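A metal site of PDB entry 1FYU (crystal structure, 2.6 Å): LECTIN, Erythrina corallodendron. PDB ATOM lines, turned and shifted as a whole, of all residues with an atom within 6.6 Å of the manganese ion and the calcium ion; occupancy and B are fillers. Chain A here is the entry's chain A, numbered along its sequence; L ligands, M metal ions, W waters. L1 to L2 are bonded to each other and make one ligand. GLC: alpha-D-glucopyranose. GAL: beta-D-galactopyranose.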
ATOM      1  N   ASP A  89     -23.114   9.112  -5.197  1.00  0.00           N
ATOM      2  CA  ASP A  89     -23.646   9.874  -6.312  1.00  0.00           C
ATOM      3  C   ASP A  89     -23.049   9.456  -7.654  1.00  0.00           C
ATOM      4  O   ASP A  89     -23.697   9.559  -8.696  1.00  0.00           O
ATOM      5  CB  ASP A  89     -23.408  11.372  -6.076  1.00  0.00           C
ATOM      6  CG  ASP A  89     -24.583  12.060  -5.380  1.00  0.00           C
ATOM      7  OD1 ASP A  89     -24.536  12.251  -4.137  1.00  0.00           O
ATOM      8  OD2 ASP A  89     -25.557  12.403  -6.081  1.00  0.00           O
ATOM      9  N   TYR A 106     -21.675  15.617  -3.616  1.00  0.00           N
ATOM     10  CA  TYR A 106     -22.963  15.046  -4.015  1.00  0.00           C
ATOM     11  C   TYR A 106     -23.097  14.988  -5.535  1.00  0.00           C
ATOM     12  O   TYR A 106     -22.157  14.597  -6.226  1.00  0.00           O
ATOM     13  CB  TYR A 106     -24.123  15.845  -3.409  1.00  0.00           C
ATOM     14  CG  TYR A 106     -23.938  16.140  -1.939  1.00  0.00           C
ATOM     15  CD1 TYR A 106     -23.428  15.179  -1.064  1.00  0.00           C
ATOM     16  CD2 TYR A 106     -24.216  17.413  -1.425  1.00  0.00           C
ATOM     17  CE1 TYR A 106     -23.192  15.476   0.284  1.00  0.00           C
ATOM     18  CE2 TYR A 106     -23.983  17.723  -0.079  1.00  0.00           C
ATOM     19  CZ  TYR A 106     -23.464  16.755   0.754  1.00  0.00           C
ATOM     20  OH  TYR A 106     -23.184  17.063   2.073  1.00  0.00           O
ATOM     21  N   GLY A 107     -24.263  15.372  -6.044  1.00  0.00           N
ATOM     22  CA  GLY A 107     -24.516  15.336  -7.471  1.00  0.00           C
ATOM     23  C   GLY A 107     -23.570  16.157  -8.335  1.00  0.00           C
ATOM     24  O   GLY A 107     -23.582  16.037  -9.557  1.00  0.00           O
ATOM     25  N   TYR A 108     -22.768  17.015  -7.708  1.00  0.00           N
ATOM     26  CA  TYR A 108     -21.833  17.839  -8.467  1.00  0.00           C
ATOM     27  C   TYR A 108     -20.520  17.083  -8.659  1.00  0.00           C
ATOM     28  O   TYR A 108     -19.574  17.584  -9.274  1.00  0.00           O
ATOM     29  CB  TYR A 108     -21.618  19.172  -7.745  1.00  0.00           C
ATOM     30  CG  TYR A 108     -22.917  19.930  -7.597  1.00  0.00           C
ATOM     31  CD1 TYR A 108     -23.565  20.446  -8.713  1.00  0.00           C
ATOM     32  CD2 TYR A 108     -23.517  20.071  -6.347  1.00  0.00           C
ATOM     33  CE1 TYR A 108     -24.790  21.081  -8.598  1.00  0.00           C
ATOM     34  CE2 TYR A 108     -24.754  20.706  -6.221  1.00  0.00           C
ATOM     35  CZ  TYR A 108     -25.379  21.203  -7.346  1.00  0.00           C
ATOM     36  OH  TYR A 108     -26.607  21.814  -7.236  1.00  0.00           O
ATOM     37  N   LEU A 109     -20.489  15.861  -8.126  1.00  0.00           N
ATOM     38  CA  LEU A 109     -19.347  14.957  -8.241  1.00  0.00           C
ATOM     39  C   LEU A 109     -17.973  15.548  -7.910  1.00  0.00           C
ATOM     40  O   LEU A 109     -16.951  14.963  -8.257  1.00  0.00           O
ATOM     41  CB  LEU A 109     -19.346  14.347  -9.643  1.00  0.00           C
ATOM     42  CG  LEU A 109     -20.678  13.675 -10.023  1.00  0.00           C
ATOM     43  CD1 LEU A 109     -20.606  13.171 -11.449  1.00  0.00           C
ATOM     44  CD2 LEU A 109     -20.989  12.528  -9.078  1.00  0.00           C
ATOM     45  N   GLU A 127     -18.900  11.232 -16.981  1.00  0.00           N
ATOM     46  CA  GLU A 127     -19.406  10.757 -15.707  1.00  0.00           C
ATOM     47  C   GLU A 127     -20.108   9.396 -15.747  1.00  0.00           C
ATOM     48  O   GLU A 127     -20.565   8.920 -16.797  1.00  0.00           O
ATOM     49  CB  GLU A 127     -20.393  11.795 -15.158  1.00  0.00           C
ATOM     50  CG  GLU A 127     -21.690  11.850 -15.957  1.00  0.00           C
ATOM     51  CD  GLU A 127     -22.708  12.825 -15.399  1.00  0.00           C
ATOM     52  OE1 GLU A 127     -23.911  12.583 -15.605  1.00  0.00           O
ATOM     53  OE2 GLU A 127     -22.316  13.842 -14.784  1.00  0.00           O
ATOM     54  N   ASP A 129     -22.815   8.456 -13.458  1.00  0.00           N
ATOM     55  CA  ASP A 129     -23.798   8.971 -12.511  1.00  0.00           C
ATOM     56  C   ASP A 129     -24.745   7.887 -12.001  1.00  0.00           C
ATOM     57  O   ASP A 129     -25.398   7.213 -12.793  1.00  0.00           O
ATOM     58  CB  ASP A 129     -24.611  10.060 -13.228  1.00  0.00           C
ATOM     59  CG  ASP A 129     -25.270  11.006 -12.278  1.00  0.00           C
ATOM     60  OD1 ASP A 129     -25.592  10.586 -11.146  1.00  0.00           O
ATOM     61  OD2 ASP A 129     -25.496  12.171 -12.658  1.00  0.00           O
ATOM     62  N   THR A 130     -24.823   7.749 -10.686  1.00  0.00           N
ATOM     63  CA  THR A 130     -25.678   6.734 -10.080  1.00  0.00           C
ATOM     64  C   THR A 130     -26.923   7.282  -9.384  1.00  0.00           C
ATOM     65  O   THR A 130     -27.742   6.498  -8.877  1.00  0.00           O
ATOM     66  CB  THR A 130     -24.894   5.878  -9.081  1.00  0.00           C
ATOM     67  OG1 THR A 130     -24.410   6.702  -8.020  1.00  0.00           O
ATOM     68  CG2 THR A 130     -23.724   5.183  -9.774  1.00  0.00           C
ATOM     69  N   PHE A 131     -27.070   8.594  -9.332  1.00  0.00           N
ATOM     70  CA  PHE A 131     -28.226   9.201  -8.693  1.00  0.00           C
ATOM     71  C   PHE A 131     -28.841  10.258  -9.606  1.00  0.00           C
ATOM     72  O   PHE A 131     -28.151  11.100 -10.160  1.00  0.00           O
ATOM     73  CB  PHE A 131     -27.847   9.822  -7.355  1.00  0.00           C
ATOM     74  CG  PHE A 131     -29.006  10.427  -6.611  1.00  0.00           C
ATOM     75  CD1 PHE A 131     -29.453  11.714  -6.917  1.00  0.00           C
ATOM     76  CD2 PHE A 131     -29.686   9.683  -5.646  1.00  0.00           C
ATOM     77  CE1 PHE A 131     -30.567  12.258  -6.269  1.00  0.00           C
ATOM     78  CE2 PHE A 131     -30.804  10.222  -4.986  1.00  0.00           C
ATOM     79  CZ  PHE A 131     -31.245  11.517  -5.294  1.00  0.00           C
ATOM     80  N   SER A 132     -30.163  10.219  -9.738  1.00  0.00           N
ATOM     81  CA  SER A 132     -30.858  11.157 -10.603  1.00  0.00           C
ATOM     82  C   SER A 132     -31.260  12.480  -9.960  1.00  0.00           C
ATOM     83  O   SER A 132     -32.254  12.558  -9.233  1.00  0.00           O
ATOM     84  CB  SER A 132     -32.101  10.487 -11.182  1.00  0.00           C
ATOM     85  OG  SER A 132     -32.693  11.341 -12.134  1.00  0.00           O
ATOM     86  N   ASN A 133     -30.485  13.527 -10.242  1.00  0.00           N
ATOM     87  CA  ASN A 133     -30.768  14.847  -9.708  1.00  0.00           C
ATOM     88  C   ASN A 133     -31.780  15.560 -10.623  1.00  0.00           C
ATOM     89  O   ASN A 133     -32.203  15.009 -11.640  1.00  0.00           O
ATOM     90  CB  ASN A 133     -29.481  15.679  -9.627  1.00  0.00           C
ATOM     91  CG  ASN A 133     -28.442  15.042  -8.733  1.00  0.00           C
ATOM     92  OD1 ASN A 133     -27.737  14.124  -9.147  1.00  0.00           O
ATOM     93  ND2 ASN A 133     -28.339  15.515  -7.500  1.00  0.00           N
ATOM     94  N   TRP A 135     -31.393  17.820 -12.763  1.00  0.00           N
ATOM     95  CA  TRP A 135     -30.847  18.010 -14.101  1.00  0.00           C
ATOM     96  C   TRP A 135     -30.532  16.715 -14.842  1.00  0.00           C
ATOM     97  O   TRP A 135     -30.098  16.744 -15.984  1.00  0.00           O
ATOM     98  CB  TRP A 135     -29.576  18.855 -14.011  1.00  0.00           C
ATOM     99  CG  TRP A 135     -28.543  18.263 -13.106  1.00  0.00           C
ATOM    100  CD1 TRP A 135     -27.681  17.240 -13.403  1.00  0.00           C
ATOM    101  CD2 TRP A 135     -28.303  18.602 -11.736  1.00  0.00           C
ATOM    102  NE1 TRP A 135     -26.913  16.924 -12.308  1.00  0.00           N
ATOM    103  CE2 TRP A 135     -27.276  17.738 -11.265  1.00  0.00           C
ATOM    104  CE3 TRP A 135     -28.848  19.537 -10.851  1.00  0.00           C
ATOM    105  CZ2 TRP A 135     -26.791  17.795  -9.947  1.00  0.00           C
ATOM    106  CZ3 TRP A 135     -28.363  19.594  -9.533  1.00  0.00           C
ATOM    107  CH2 TRP A 135     -27.341  18.721  -9.101  1.00  0.00           C
ATOM    108  N   ASP A 136     -30.759  15.580 -14.190  1.00  0.00           N
ATOM    109  CA  ASP A 136     -30.477  14.276 -14.790  1.00  0.00           C
ATOM    110  C   ASP A 136     -31.670  13.641 -15.466  1.00  0.00           C
ATOM    111  O   ASP A 136     -32.811  14.027 -15.213  1.00  0.00           O
ATOM    112  CB  ASP A 136     -29.992  13.280 -13.729  1.00  0.00           C
ATOM    113  CG  ASP A 136     -28.574  13.525 -13.294  1.00  0.00           C
ATOM    114  OD1 ASP A 136     -27.704  13.618 -14.178  1.00  0.00           O
ATOM    115  OD2 ASP A 136     -28.319  13.594 -12.072  1.00  0.00           O
ATOM    116  N   PRO A 137     -31.420  12.678 -16.357  1.00  0.00           N
ATOM    117  CA  PRO A 137     -32.530  11.990 -17.022  1.00  0.00           C
ATOM    118  C   PRO A 137     -33.057  11.063 -15.921  1.00  0.00           C
ATOM    119  O   PRO A 137     -32.426  10.936 -14.871  1.00  0.00           O
ATOM    120  CB  PRO A 137     -31.835  11.237 -18.155  1.00  0.00           C
ATOM    121  CG  PRO A 137     -30.448  10.988 -17.614  1.00  0.00           C
ATOM    122  CD  PRO A 137     -30.129  12.311 -16.976  1.00  0.00           C
ATOM    123  N   VAL A 140     -30.761   5.718 -14.125  1.00  0.00           N
ATOM    124  CA  VAL A 140     -29.465   5.640 -13.476  1.00  0.00           C
ATOM    125  C   VAL A 140     -29.148   4.174 -13.226  1.00  0.00           C
ATOM    126  O   VAL A 140     -30.035   3.354 -13.053  1.00  0.00           O
ATOM    127  CB  VAL A 140     -29.433   6.423 -12.128  1.00  0.00           C
ATOM    128  CG1 VAL A 140     -29.589   7.914 -12.394  1.00  0.00           C
ATOM    129  CG2 VAL A 140     -30.515   5.924 -11.205  1.00  0.00           C
ATOM    130  N   HIS A 142     -26.003   6.116 -15.399  1.00  0.00           N
ATOM    131  CA  HIS A 142     -25.890   6.503 -16.796  1.00  0.00           C
ATOM    132  C   HIS A 142     -24.520   7.110 -17.048  1.00  0.00           C
ATOM    133  O   HIS A 142     -23.890   7.662 -16.142  1.00  0.00           O
ATOM    134  CB  HIS A 142     -26.987   7.499 -17.195  1.00  0.00           C
ATOM    135  CG  HIS A 142     -26.962   8.799 -16.429  1.00  0.00           C
ATOM    136  ND1 HIS A 142     -27.931   9.135 -15.505  1.00  0.00           N
ATOM    137  CD2 HIS A 142     -26.098   9.841 -16.463  1.00  0.00           C
ATOM    138  CE1 HIS A 142     -27.664  10.323 -15.005  1.00  0.00           C
ATOM    139  NE2 HIS A 142     -26.555  10.782 -15.570  1.00  0.00           N
ATOM    140  N   ILE A 143     -24.050   6.974 -18.281  1.00  0.00           N
ATOM    141  CA  ILE A 143     -22.783   7.566 -18.680  1.00  0.00           C
ATOM    142  C   ILE A 143     -23.226   8.907 -19.237  1.00  0.00           C
ATOM    143  O   ILE A 143     -24.288   9.011 -19.861  1.00  0.00           O
ATOM    144  CB  ILE A 143     -22.085   6.764 -19.803  1.00  0.00           C
ATOM    145  CG1 ILE A 143     -21.937   5.301 -19.386  1.00  0.00           C
ATOM    146  CG2 ILE A 143     -20.721   7.379 -20.118  1.00  0.00           C
ATOM    147  CD1 ILE A 143     -21.343   4.417 -20.476  1.00  0.00           C
ATOM    148  N   GLY A 144     -22.439   9.949 -19.002  1.00  0.00           N
ATOM    149  CA  GLY A 144     -22.800  11.252 -19.508  1.00  0.00           C
ATOM    150  C   GLY A 144     -21.564  12.033 -19.885  1.00  0.00           C
ATOM    151  O   GLY A 144     -20.509  11.900 -19.253  1.00  0.00           O
ATOM    152  N   ASP A 146     -19.990  15.545 -19.978  1.00  0.00           N
ATOM    153  CA  ASP A 146     -20.148  16.856 -19.366  1.00  0.00           C
ATOM    154  C   ASP A 146     -19.231  17.928 -19.932  1.00  0.00           C
ATOM    155  O   ASP A 146     -18.009  17.836 -19.797  1.00  0.00           O
ATOM    156  CB  ASP A 146     -19.941  16.752 -17.850  1.00  0.00           C
ATOM    157  CG  ASP A 146     -20.948  15.834 -17.183  1.00  0.00           C
ATOM    158  OD1 ASP A 146     -21.941  15.448 -17.829  1.00  0.00           O
ATOM    159  OD2 ASP A 146     -20.747  15.516 -16.000  1.00  0.00           O
ATOM    160  N   ILE A 150     -22.748  20.105 -15.243  1.00  0.00           N
ATOM    161  CA  ILE A 150     -23.114  18.813 -14.713  1.00  0.00           C
ATOM    162  C   ILE A 150     -24.317  18.323 -15.503  1.00  0.00           C
ATOM    163  O   ILE A 150     -24.666  17.151 -15.458  1.00  0.00           O
ATOM    164  CB  ILE A 150     -23.500  18.901 -13.222  1.00  0.00           C
ATOM    165  CG1 ILE A 150     -23.564  17.504 -12.615  1.00  0.00           C
ATOM    166  CG2 ILE A 150     -24.848  19.604 -13.075  1.00  0.00           C
ATOM    167  CD1 ILE A 150     -22.229  16.765 -12.628  1.00  0.00           C
ATOM    168  N   ARG A 151     -24.961  19.232 -16.234  1.00  0.00           N
ATOM    169  CA  ARG A 151     -26.108  18.844 -17.055  1.00  0.00           C
ATOM    170  C   ARG A 151     -25.513  18.369 -18.383  1.00  0.00           C
ATOM    171  O   ARG A 151     -25.216  19.171 -19.268  1.00  0.00           O
ATOM    172  CB  ARG A 151     -27.054  20.034 -17.271  1.00  0.00           C
ATOM    173  CG  ARG A 151     -28.284  19.665 -18.085  1.00  0.00           C
ATOM    174  CD  ARG A 151     -29.218  20.835 -18.380  1.00  0.00           C
ATOM    175  NE  ARG A 151     -30.277  21.001 -17.395  1.00  0.00           N
ATOM    176  CZ  ARG A 151     -30.177  21.737 -16.283  1.00  0.00           C
ATOM    177  NH1 ARG A 151     -29.051  22.387 -16.015  1.00  0.00           N
ATOM    178  NH2 ARG A 151     -31.210  21.813 -15.447  1.00  0.00           N
ATOM    179  N   SER A 152     -25.317  17.056 -18.493  1.00  0.00           N
ATOM    180  CA  SER A 152     -24.730  16.411 -19.667  1.00  0.00           C
ATOM    181  C   SER A 152     -25.349  16.802 -20.997  1.00  0.00           C
ATOM    182  O   SER A 152     -26.550  17.036 -21.073  1.00  0.00           O
ATOM    183  CB  SER A 152     -24.832  14.892 -19.524  1.00  0.00           C
ATOM    184  OG  SER A 152     -24.244  14.433 -18.320  1.00  0.00           O
ATOM    185  N   THR A 155     -26.347  11.580 -22.940  1.00  0.00           N
ATOM    186  CA  THR A 155     -26.502  10.599 -21.888  1.00  0.00           C
ATOM    187  C   THR A 155     -26.766   9.180 -22.398  1.00  0.00           C
ATOM    188  O   THR A 155     -27.446   9.002 -23.414  1.00  0.00           O
ATOM    189  CB  THR A 155     -27.648  11.067 -20.960  1.00  0.00           C
ATOM    190  OG1 THR A 155     -27.083  11.582 -19.758  1.00  0.00           O
ATOM    191  CG2 THR A 155     -28.630   9.960 -20.678  1.00  0.00           C
HETATM  192  C1  GLC L   1     -32.555  16.965   1.443  1.00  0.00           C
HETATM  193  C2  GLC L   1     -32.069  15.514   1.511  1.00  0.00           C
HETATM  194  C3  GLC L   1     -30.776  15.360   0.708  1.00  0.00           C
HETATM  195  C4  GLC L   1     -30.968  15.867  -0.726  1.00  0.00           C
HETATM  196  C5  GLC L   1     -31.576  17.281  -0.738  1.00  0.00           C
HETATM  197  C6  GLC L   1     -31.986  17.694  -2.142  1.00  0.00           C
HETATM  198  O1  GLC L   1     -31.568  17.808   1.944  1.00  0.00           O
HETATM  199  O2  GLC L   1     -31.838  15.155   2.865  1.00  0.00           O
HETATM  200  O3  GLC L   1     -30.402  13.991   0.680  1.00  0.00           O
HETATM  201  O4  GLC L   1     -29.699  15.878  -1.418  1.00  0.00           O
HETATM  202  O5  GLC L   1     -32.784  17.327   0.067  1.00  0.00           O
HETATM  203  O6  GLC L   1     -31.617  19.035  -2.395  1.00  0.00           O
HETATM  204  C1  GAL L   2     -29.529  14.902  -2.398  1.00  0.00           C
HETATM  205  C2  GAL L   2     -28.340  15.275  -3.296  1.00  0.00           C
HETATM  206  C3  GAL L   2     -28.054  14.128  -4.294  1.00  0.00           C
HETATM  207  C4  GAL L   2     -27.895  12.798  -3.558  1.00  0.00           C
HETATM  208  C5  GAL L   2     -29.117  12.556  -2.674  1.00  0.00           C
HETATM  209  C6  GAL L   2     -29.013  11.290  -1.851  1.00  0.00           C
HETATM  210  O2  GAL L   2     -28.637  16.470  -4.004  1.00  0.00           O
HETATM  211  O3  GAL L   2     -26.869  14.410  -5.016  1.00  0.00           O
HETATM  212  O4  GAL L   2     -26.725  12.842  -2.754  1.00  0.00           O
HETATM  213  O5  GAL L   2     -29.274  13.659  -1.735  1.00  0.00           O
HETATM  214  O6  GAL L   2     -30.118  11.150  -0.987  1.00  0.00           O
HETATM  215 MN    MN M   1     -25.894  12.838 -14.763  1.00  0.00          MN
HETATM  216 CA    CA M   2     -26.666  12.792 -10.634  1.00  0.00          CA
HETATM  217  O   HOH W   1     -24.800  14.627 -13.923  1.00  0.00           O
HETATM  218  O   HOH W   2     -25.033  14.561 -11.145  1.00  0.00           O
HETATM  219  O   HOH W   3     -26.286  13.792 -16.624  1.00  0.00           O
HETATM  220  O   HOH W   4     -25.293  12.264  -8.775  1.00  0.00           O
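Four residues have an atom within 4 Å of the manganese ion: Glu 127, Asp 129, Asp 136 and His 142. The nearest printed residue that does not touch the manganese ion is Ser 152 (4.2 Å).
OG of Ser 152 sits close to OE1 of Glu 127 (3.3 Å). OE2 of Glu 127 sits close to OD2 of Asp 146, at 2.6 Å. The backbone carbonyl oxygen (O) of Gly 144 is in hydrogen-bond range of the backbone NH (N) of Glu 127 (2.9 Å).
Within 4 Å of the calcium ion: Asp 129, Phe 131, Asn 133 and Asp 136.
Water W1 bridges the side-chain carboxylate of Glu 127 and the backbone carbonyl oxygen of Ile 150. Water W2 lies within hydrogen-bond range of O of Gly 107 (2.6 Å) and NE1 of Trp 135 (3.2 Å).
The calcium ion is bound by OD1 of Asn 133, O of Phe 131, OD2 of Asp 136, water W4, OD2 of Asp 129, water W2 and OD1 of Asp 129. The calcium ion has seven donor atoms within binding distance.
The manganese ion is bound by the side-chain carboxylate (OD1) of Asp 136 (2.1 Å). The manganese ion is bound by water W3. OE1 of Glu 127 is bound to the manganese ion. OD2 of Asp 129 is bound to the manganese ion, at 2.2 Å. The manganese ion is bound by water W1. NE2 of His 142 binds the manganese ion (2.3 Å). The manganese ion has six donor atoms within binding distance.
An oxygen (O3) of GAL L2 is in hydrogen-bond range of the side-chain amide nitrogen of Asn 133. N of Gly 107 sits at hydrogen-bond distance from O3 of GAL L2, 3.0 Å away. An oxygen (O3) of GAL L2 lies within hydrogen-bond range of the side-chain carboxylate (OD2) of Asp 89, at 2.6 Å.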
